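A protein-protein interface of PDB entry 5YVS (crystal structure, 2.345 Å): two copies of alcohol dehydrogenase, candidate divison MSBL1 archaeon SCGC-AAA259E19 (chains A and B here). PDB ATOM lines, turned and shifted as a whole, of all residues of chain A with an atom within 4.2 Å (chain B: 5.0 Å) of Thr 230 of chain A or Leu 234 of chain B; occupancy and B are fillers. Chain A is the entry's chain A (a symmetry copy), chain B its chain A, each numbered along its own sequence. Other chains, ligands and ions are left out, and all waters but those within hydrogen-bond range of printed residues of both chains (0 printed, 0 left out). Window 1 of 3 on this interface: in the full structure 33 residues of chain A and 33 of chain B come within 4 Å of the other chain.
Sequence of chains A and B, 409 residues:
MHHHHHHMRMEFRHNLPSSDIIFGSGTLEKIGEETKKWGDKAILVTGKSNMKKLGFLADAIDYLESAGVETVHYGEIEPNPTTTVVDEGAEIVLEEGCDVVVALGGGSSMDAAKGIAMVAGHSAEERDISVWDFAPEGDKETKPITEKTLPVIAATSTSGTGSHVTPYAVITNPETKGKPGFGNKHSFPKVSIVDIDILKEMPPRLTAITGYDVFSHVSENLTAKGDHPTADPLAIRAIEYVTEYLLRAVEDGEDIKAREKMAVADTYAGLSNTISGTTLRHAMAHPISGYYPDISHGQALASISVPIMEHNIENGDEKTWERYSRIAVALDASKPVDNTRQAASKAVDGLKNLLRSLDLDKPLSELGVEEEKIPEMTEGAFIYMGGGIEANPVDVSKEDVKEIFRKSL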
ATOM      1  N   HIS A  14      17.056 -14.040  -0.956  1.00  0.00           N
ATOM      2  CA  HIS A  14      15.859 -14.832  -0.705  1.00  0.00           C
ATOM      3  C   HIS A  14      14.715 -14.312  -1.566  1.00  0.00           C
ATOM      4  O   HIS A  14      14.385 -13.122  -1.512  1.00  0.00           O
ATOM      5  CB  HIS A  14      15.490 -14.771   0.782  1.00  0.00           C
ATOM      6  CG  HIS A  14      14.053 -15.081   1.076  1.00  0.00           C
ATOM      7  ND1 HIS A  14      13.650 -16.272   1.640  1.00  0.00           N
ATOM      8  CD2 HIS A  14      12.927 -14.345   0.911  1.00  0.00           C
ATOM      9  CE1 HIS A  14      12.339 -16.264   1.796  1.00  0.00           C
ATOM     10  NE2 HIS A  14      11.874 -15.108   1.359  1.00  0.00           N
ATOM     11  N   HIS A 228      21.503 -20.418   2.389  1.00  0.00           N
ATOM     12  CA  HIS A 228      20.059 -20.299   2.211  1.00  0.00           C
ATOM     13  C   HIS A 228      19.359 -20.507   3.549  1.00  0.00           C
ATOM     14  O   HIS A 228      18.555 -21.436   3.694  1.00  0.00           O
ATOM     15  CB  HIS A 228      19.552 -21.304   1.176  1.00  0.00           C
ATOM     16  CG  HIS A 228      20.350 -22.569   1.116  1.00  0.00           C
ATOM     17  ND1 HIS A 228      20.351 -23.503   2.131  1.00  0.00           N
ATOM     18  CD2 HIS A 228      21.175 -23.056   0.157  1.00  0.00           C
ATOM     19  CE1 HIS A 228      21.140 -24.509   1.800  1.00  0.00           C
ATOM     20  NE2 HIS A 228      21.652 -24.262   0.607  1.00  0.00           N
ATOM     21  N   PRO A 229      19.626 -19.653   4.543  1.00  0.00           N
ATOM     22  CA  PRO A 229      19.134 -19.929   5.903  1.00  0.00           C
ATOM     23  C   PRO A 229      17.633 -19.777   6.068  1.00  0.00           C
ATOM     24  O   PRO A 229      17.091 -20.278   7.062  1.00  0.00           O
ATOM     25  CB  PRO A 229      19.891 -18.910   6.765  1.00  0.00           C
ATOM     26  CG  PRO A 229      20.229 -17.802   5.831  1.00  0.00           C
ATOM     27  CD  PRO A 229      20.437 -18.426   4.479  1.00  0.00           C
ATOM     28  N   THR A 230      16.941 -19.103   5.149  1.00  0.00           N
ATOM     29  CA  THR A 230      15.497 -18.962   5.280  1.00  0.00           C
ATOM     30  C   THR A 230      14.754 -20.258   4.977  1.00  0.00           C
ATOM     31  O   THR A 230      13.626 -20.434   5.449  1.00  0.00           O
ATOM     32  CB  THR A 230      14.990 -17.841   4.371  1.00  0.00           C
ATOM     33  OG1 THR A 230      15.361 -18.114   3.016  1.00  0.00           O
ATOM     34  CG2 THR A 230      15.599 -16.518   4.787  1.00  0.00           C
ATOM     35  N   ALA A 231      15.362 -21.174   4.226  1.00  0.00           N
ATOM     36  CA  ALA A 231      14.739 -22.466   3.975  1.00  0.00           C
ATOM     37  C   ALA A 231      15.168 -23.536   4.967  1.00  0.00           C
ATOM     38  O   ALA A 231      14.419 -24.491   5.182  1.00  0.00           O
ATOM     39  CB  ALA A 231      15.042 -22.937   2.547  1.00  0.00           C
ATOM     40  N   ASP A 232      16.341 -23.403   5.583  1.00  0.00           N
ATOM     41  CA  ASP A 232      16.894 -24.518   6.351  1.00  0.00           C
ATOM     42  C   ASP A 232      15.994 -24.980   7.491  1.00  0.00           C
ATOM     43  O   ASP A 232      15.770 -26.197   7.613  1.00  0.00           O
ATOM     44  CB  ASP A 232      18.297 -24.159   6.855  1.00  0.00           C
ATOM     45  CG  ASP A 232      19.288 -23.927   5.721  1.00  0.00           C
ATOM     46  OD1 ASP A 232      18.952 -24.257   4.560  1.00  0.00           O
ATOM     47  OD2 ASP A 232      20.393 -23.393   5.983  1.00  0.00           O
ATOM     48  N   PRO A 233      15.448 -24.106   8.348  1.00  0.00           N
ATOM     49  CA  PRO A 233      14.585 -24.623   9.427  1.00  0.00           C
ATOM     50  C   PRO A 233      13.393 -25.408   8.912  1.00  0.00           C
ATOM     51  O   PRO A 233      13.039 -26.441   9.494  1.00  0.00           O
ATOM     52  CB  PRO A 233      14.144 -23.354  10.176  1.00  0.00           C
ATOM     53  CG  PRO A 233      15.175 -22.342   9.822  1.00  0.00           C
ATOM     54  CD  PRO A 233      15.586 -22.642   8.417  1.00  0.00           C
ATOM     55  N   ILE A 275      12.739 -21.385  -2.292  1.00  0.00           N
ATOM     56  CA  ILE A 275      13.821 -20.530  -1.811  1.00  0.00           C
ATOM     57  C   ILE A 275      15.175 -21.082  -2.239  1.00  0.00           C
ATOM     58  O   ILE A 275      16.029 -20.350  -2.754  1.00  0.00           O
ATOM     59  CB  ILE A 275      13.741 -20.384  -0.281  1.00  0.00           C
ATOM     60  CG1 ILE A 275      12.439 -19.687   0.125  1.00  0.00           C
ATOM     61  CG2 ILE A 275      14.956 -19.638   0.248  1.00  0.00           C
ATOM     62  CD1 ILE A 275      12.104 -19.845   1.592  1.00  0.00           C
ATOM     63  N   ILE B  21      14.685 -10.591  -0.327  1.00  0.00           N
ATOM     64  CA  ILE B  21      15.651 -10.246   0.712  1.00  0.00           C
ATOM     65  C   ILE B  21      17.053 -10.319   0.121  1.00  0.00           C
ATOM     66  O   ILE B  21      17.462 -11.366  -0.397  1.00  0.00           O
ATOM     67  CB  ILE B  21      15.521 -11.170   1.934  1.00  0.00           C
ATOM     68  CG1 ILE B  21      14.079 -11.178   2.443  1.00  0.00           C
ATOM     69  CG2 ILE B  21      16.467 -10.729   3.037  1.00  0.00           C
ATOM     70  CD1 ILE B  21      13.829 -12.130   3.588  1.00  0.00           C
ATOM     71  N   VAL B 218       9.357 -14.020  18.183  1.00  0.00           N
ATOM     72  CA  VAL B 218       9.269 -15.446  17.893  1.00  0.00           C
ATOM     73  C   VAL B 218       8.669 -16.216  19.064  1.00  0.00           C
ATOM     74  O   VAL B 218       7.912 -17.173  18.857  1.00  0.00           O
ATOM     75  CB  VAL B 218      10.655 -15.989  17.498  1.00  0.00           C
ATOM     76  CG1 VAL B 218      11.081 -15.406  16.164  1.00  0.00           C
ATOM     77  CG2 VAL B 218      11.673 -15.653  18.563  1.00  0.00           C
ATOM     78  N   THR B 230       3.782 -23.163   9.781  1.00  0.00           N
ATOM     79  CA  THR B 230       4.714 -22.599   8.813  1.00  0.00           C
ATOM     80  C   THR B 230       5.654 -21.574   9.437  1.00  0.00           C
ATOM     81  O   THR B 230       6.741 -21.340   8.898  1.00  0.00           O
ATOM     82  CB  THR B 230       3.951 -21.969   7.646  1.00  0.00           C
ATOM     83  OG1 THR B 230       3.053 -20.971   8.141  1.00  0.00           O
ATOM     84  CG2 THR B 230       3.151 -23.029   6.917  1.00  0.00           C
ATOM     85  N   ALA B 231       5.277 -20.975  10.566  1.00  0.00           N
ATOM     86  CA  ALA B 231       6.169 -20.053  11.255  1.00  0.00           C
ATOM     87  C   ALA B 231       7.005 -20.727  12.331  1.00  0.00           C
ATOM     88  O   ALA B 231       8.084 -20.226  12.655  1.00  0.00           O
ATOM     89  CB  ALA B 231       5.368 -18.898  11.872  1.00  0.00           C
ATOM     90  N   ASP B 232       6.550 -21.848  12.886  1.00  0.00           N
ATOM     91  CA  ASP B 232       7.197 -22.387  14.082  1.00  0.00           C
ATOM     92  C   ASP B 232       8.673 -22.717  13.880  1.00  0.00           C
ATOM     93  O   ASP B 232       9.489 -22.317  14.728  1.00  0.00           O
ATOM     94  CB  ASP B 232       6.416 -23.604  14.594  1.00  0.00           C
ATOM     95  CG  ASP B 232       5.002 -23.251  15.035  1.00  0.00           C
ATOM     96  OD1 ASP B 232       4.698 -22.041  15.152  1.00  0.00           O
ATOM     97  OD2 ASP B 232       4.183 -24.180  15.241  1.00  0.00           O
ATOM     98  N   PRO B 233       9.092 -23.418  12.818  1.00  0.00           N
ATOM     99  CA  PRO B 233      10.535 -23.699  12.685  1.00  0.00           C
ATOM    100  C   PRO B 233      11.385 -22.443  12.642  1.00  0.00           C
ATOM    101  O   PRO B 233      12.464 -22.409  13.246  1.00  0.00           O
ATOM    102  CB  PRO B 233      10.629 -24.490  11.370  1.00  0.00           C
ATOM    103  CG  PRO B 233       9.260 -25.036  11.171  1.00  0.00           C
ATOM    104  CD  PRO B 233       8.320 -24.008  11.712  1.00  0.00           C
ATOM    105  N   LEU B 234      10.918 -21.399  11.948  1.00  0.00           N
ATOM    106  CA  LEU B 234      11.650 -20.137  11.916  1.00  0.00           C
ATOM    107  C   LEU B 234      11.733 -19.511  13.303  1.00  0.00           C
ATOM    108  O   LEU B 234      12.792 -19.019  13.709  1.00  0.00           O
ATOM    109  CB  LEU B 234      10.985 -19.177  10.929  1.00  0.00           C
ATOM    110  CG  LEU B 234      10.773 -19.710   9.508  1.00  0.00           C
ATOM    111  CD1 LEU B 234      10.087 -18.674   8.630  1.00  0.00           C
ATOM    112  CD2 LEU B 234      12.095 -20.149   8.890  1.00  0.00           C
ATOM    113  N   ALA B 235      10.626 -19.528  14.049  1.00  0.00           N
ATOM    114  CA  ALA B 235      10.623 -18.953  15.390  1.00  0.00           C
ATOM    115  C   ALA B 235      11.569 -19.709  16.319  1.00  0.00           C
ATOM    116  O   ALA B 235      12.337 -19.097  17.071  1.00  0.00           O
ATOM    117  CB  ALA B 235       9.198 -18.944  15.948  1.00  0.00           C
ATOM    118  N   ILE B 236      11.529 -21.045  16.285  1.00  0.00           N
ATOM    119  CA  ILE B 236      12.426 -21.834  17.129  1.00  0.00           C
ATOM    120  C   ILE B 236      13.877 -21.529  16.786  1.00  0.00           C
ATOM    121  O   ILE B 236      14.703 -21.269  17.668  1.00  0.00           O
ATOM    122  CB  ILE B 236      12.126 -23.337  16.991  1.00  0.00           C
ATOM    123  CG1 ILE B 236      10.781 -23.689  17.632  1.00  0.00           C
ATOM    124  CG2 ILE B 236      13.256 -24.156  17.612  1.00  0.00           C
ATOM    125  CD1 ILE B 236      10.744 -23.496  19.131  1.00  0.00           C
ATOM    126  N   ARG B 237      14.212 -21.565  15.495  1.00  0.00           N
ATOM    127  CA  ARG B 237      15.595 -21.336  15.092  1.00  0.00           C
ATOM    128  C   ARG B 237      16.081 -19.963  15.526  1.00  0.00           C
ATOM    129  O   ARG B 237      17.271 -19.790  15.817  1.00  0.00           O
ATOM    130  CB  ARG B 237      15.734 -21.498  13.576  1.00  0.00           C
ATOM    131  CG  ARG B 237      17.171 -21.553  13.090  1.00  0.00           C
ATOM    132  CD  ARG B 237      17.914 -22.716  13.729  1.00  0.00           C
ATOM    133  NE  ARG B 237      19.199 -22.971  13.085  1.00  0.00           N
ATOM    134  CZ  ARG B 237      20.136 -23.773  13.578  1.00  0.00           C
ATOM    135  NH1 ARG B 237      21.274 -23.947  12.922  1.00  0.00           N
ATOM    136  NH2 ARG B 237      19.937 -24.395  14.732  1.00  0.00           N
ATOM    137  N   ALA B 238      15.182 -18.977  15.575  1.00  0.00           N
ATOM    138  CA  ALA B 238      15.576 -17.644  16.014  1.00  0.00           C
ATOM    139  C   ALA B 238      15.947 -17.639  17.491  1.00  0.00           C
ATOM    140  O   ALA B 238      16.950 -17.030  17.882  1.00  0.00           O
ATOM    141  CB  ALA B 238      14.455 -16.642  15.736  1.00  0.00           C
ATOM    142  N   THR B 267      15.417 -11.644  10.678  1.00  0.00           N
ATOM    143  CA  THR B 267      14.628 -11.923   9.482  1.00  0.00           C
ATOM    144  C   THR B 267      13.618 -13.034   9.743  1.00  0.00           C
ATOM    145  O   THR B 267      12.456 -12.929   9.334  1.00  0.00           O
ATOM    146  CB  THR B 267      15.552 -12.280   8.317  1.00  0.00           C
ATOM    147  OG1 THR B 267      16.351 -11.139   7.981  1.00  0.00           O
ATOM    148  CG2 THR B 267      14.745 -12.697   7.097  1.00  0.00           C
ATOM    149  N   TYR B 268      14.036 -14.099  10.436  1.00  0.00           N
ATOM    150  CA  TYR B 268      13.087 -15.122  10.865  1.00  0.00           C
ATOM    151  C   TYR B 268      11.894 -14.489  11.570  1.00  0.00           C
ATOM    152  O   TYR B 268      10.737 -14.810  11.276  1.00  0.00           O
ATOM    153  CB  TYR B 268      13.767 -16.128  11.797  1.00  0.00           C
ATOM    154  CG  TYR B 268      14.746 -17.083  11.146  1.00  0.00           C
ATOM    155  CD1 TYR B 268      14.745 -17.298   9.776  1.00  0.00           C
ATOM    156  CD2 TYR B 268      15.665 -17.784  11.915  1.00  0.00           C
ATOM    157  CE1 TYR B 268      15.642 -18.178   9.188  1.00  0.00           C
ATOM    158  CE2 TYR B 268      16.562 -18.663  11.337  1.00  0.00           C
ATOM    159  CZ  TYR B 268      16.547 -18.856   9.975  1.00  0.00           C
ATOM    160  OH  TYR B 268      17.442 -19.733   9.405  1.00  0.00           O
ATOM    161  N   LEU B 271       9.290 -12.750   9.171  1.00  0.00           N
ATOM    162  CA  LEU B 271       8.451 -13.713   8.467  1.00  0.00           C
ATOM    163  C   LEU B 271       7.509 -14.421   9.429  1.00  0.00           C
ATOM    164  O   LEU B 271       6.321 -14.594   9.135  1.00  0.00           O
ATOM    165  CB  LEU B 271       9.325 -14.723   7.730  1.00  0.00           C
ATOM    166  CG  LEU B 271      10.288 -14.123   6.705  1.00  0.00           C
ATOM    167  CD1 LEU B 271      11.258 -15.181   6.220  1.00  0.00           C
ATOM    168  CD2 LEU B 271       9.522 -13.517   5.537  1.00  0.00           C
ATOM    169  N   SER B 272       8.022 -14.838  10.587  1.00  0.00           N
ATOM    170  CA  SER B 272       7.186 -15.501  11.583  1.00  0.00           C
ATOM    171  C   SER B 272       6.075 -14.580  12.079  1.00  0.00           C
ATOM    172  O   SER B 272       4.921 -15.002  12.210  1.00  0.00           O
ATOM    173  CB  SER B 272       8.059 -15.985  12.744  1.00  0.00           C
ATOM    174  OG  SER B 272       7.271 -16.435  13.829  1.00  0.00           O
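His 228 of chain A touches none of the printed residues of chain B. Of the printed residues of chain B, Thr 230 of chain A touches Leu 234 (3.8 Å) and Tyr 268 (3.99 Å). Of the printed residues of chain B, Pro 233 of chain A touches Pro 233, Leu 234, Arg 237 and Tyr 268. Printed residues of chain A within 4 Å of Ile 21 of chain B: His 14. Of the printed residues of chain A, Pro 233 of chain B touches Pro 233 (3.6 Å). Of chain A, only Thr 230 and Pro 233 come within 4 Å of Leu 234 of chain B. Of the printed residues of chain A, Arg 237 of chain B touches Pro 233 (3.9 Å). The nearest printed residue of chain B that does not touch Thr 230 of chain A is Thr 267 of chain B (4.5 Å).
Thr 230 of chain A touches Leu 234 of chain B. CA of Thr 230 of chain A touches CE1 of Tyr 268 of chain B (3.99 Å). O of Pro 233 of chain A touches CB of Pro 233 of chain B (3.6 Å). Pro 233 of chain A touches Leu 234 of chain B. CB of Arg 237 of chain B touches CG of Pro 233 of chain A (3.9 Å). Pro 233 of chain A touches Tyr 268 of chain B (CG to OH, 3.5 Å).
A ring nitrogen (ND1) of His 14 of chain A lies within hydrogen-bond range of the side-chain hydroxyl (OG1) of Thr 230 of chain A.
Pro 233 of chain A touches its own counterpart, Pro 233 of chain B. 4 positions are printed for both chains. Of the 8 pairs that touch across the chains among the printed residues, 1 has its exchanged pair printed and touching as well.
OH of Tyr 268 of chain B is in hydrogen-bond range of O of Pro 229 of chain A, at 2.4 Å. The backbone NH of His 14 of chain A lies within hydrogen-bond range of the backbone carbonyl oxygen of Ile 21 of chain B.
Of the 8 printed residues of chain A, 4 touch a printed residue of chain B. Of the 15 printed residues of chain B, 5 touch a printed residue of chain A. Printed residues of chain B that touch a printed residue of chain A: Ile 21, Pro 233, Leu 234, Arg 237 and Tyr 268. Hydrophobic or aromatic side chains of chain B within 4 Å of the printed part of chain A: Ile 21, Pro 233, Leu 234 and Tyr 268. Along chain B the printed residues that touch a printed residue of chain A span positions 21 to 268. Among the printed residues, no Asp or Glu carboxylate lies within 4 Å of a Lys or Arg side-chain nitrogen of the other chain.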
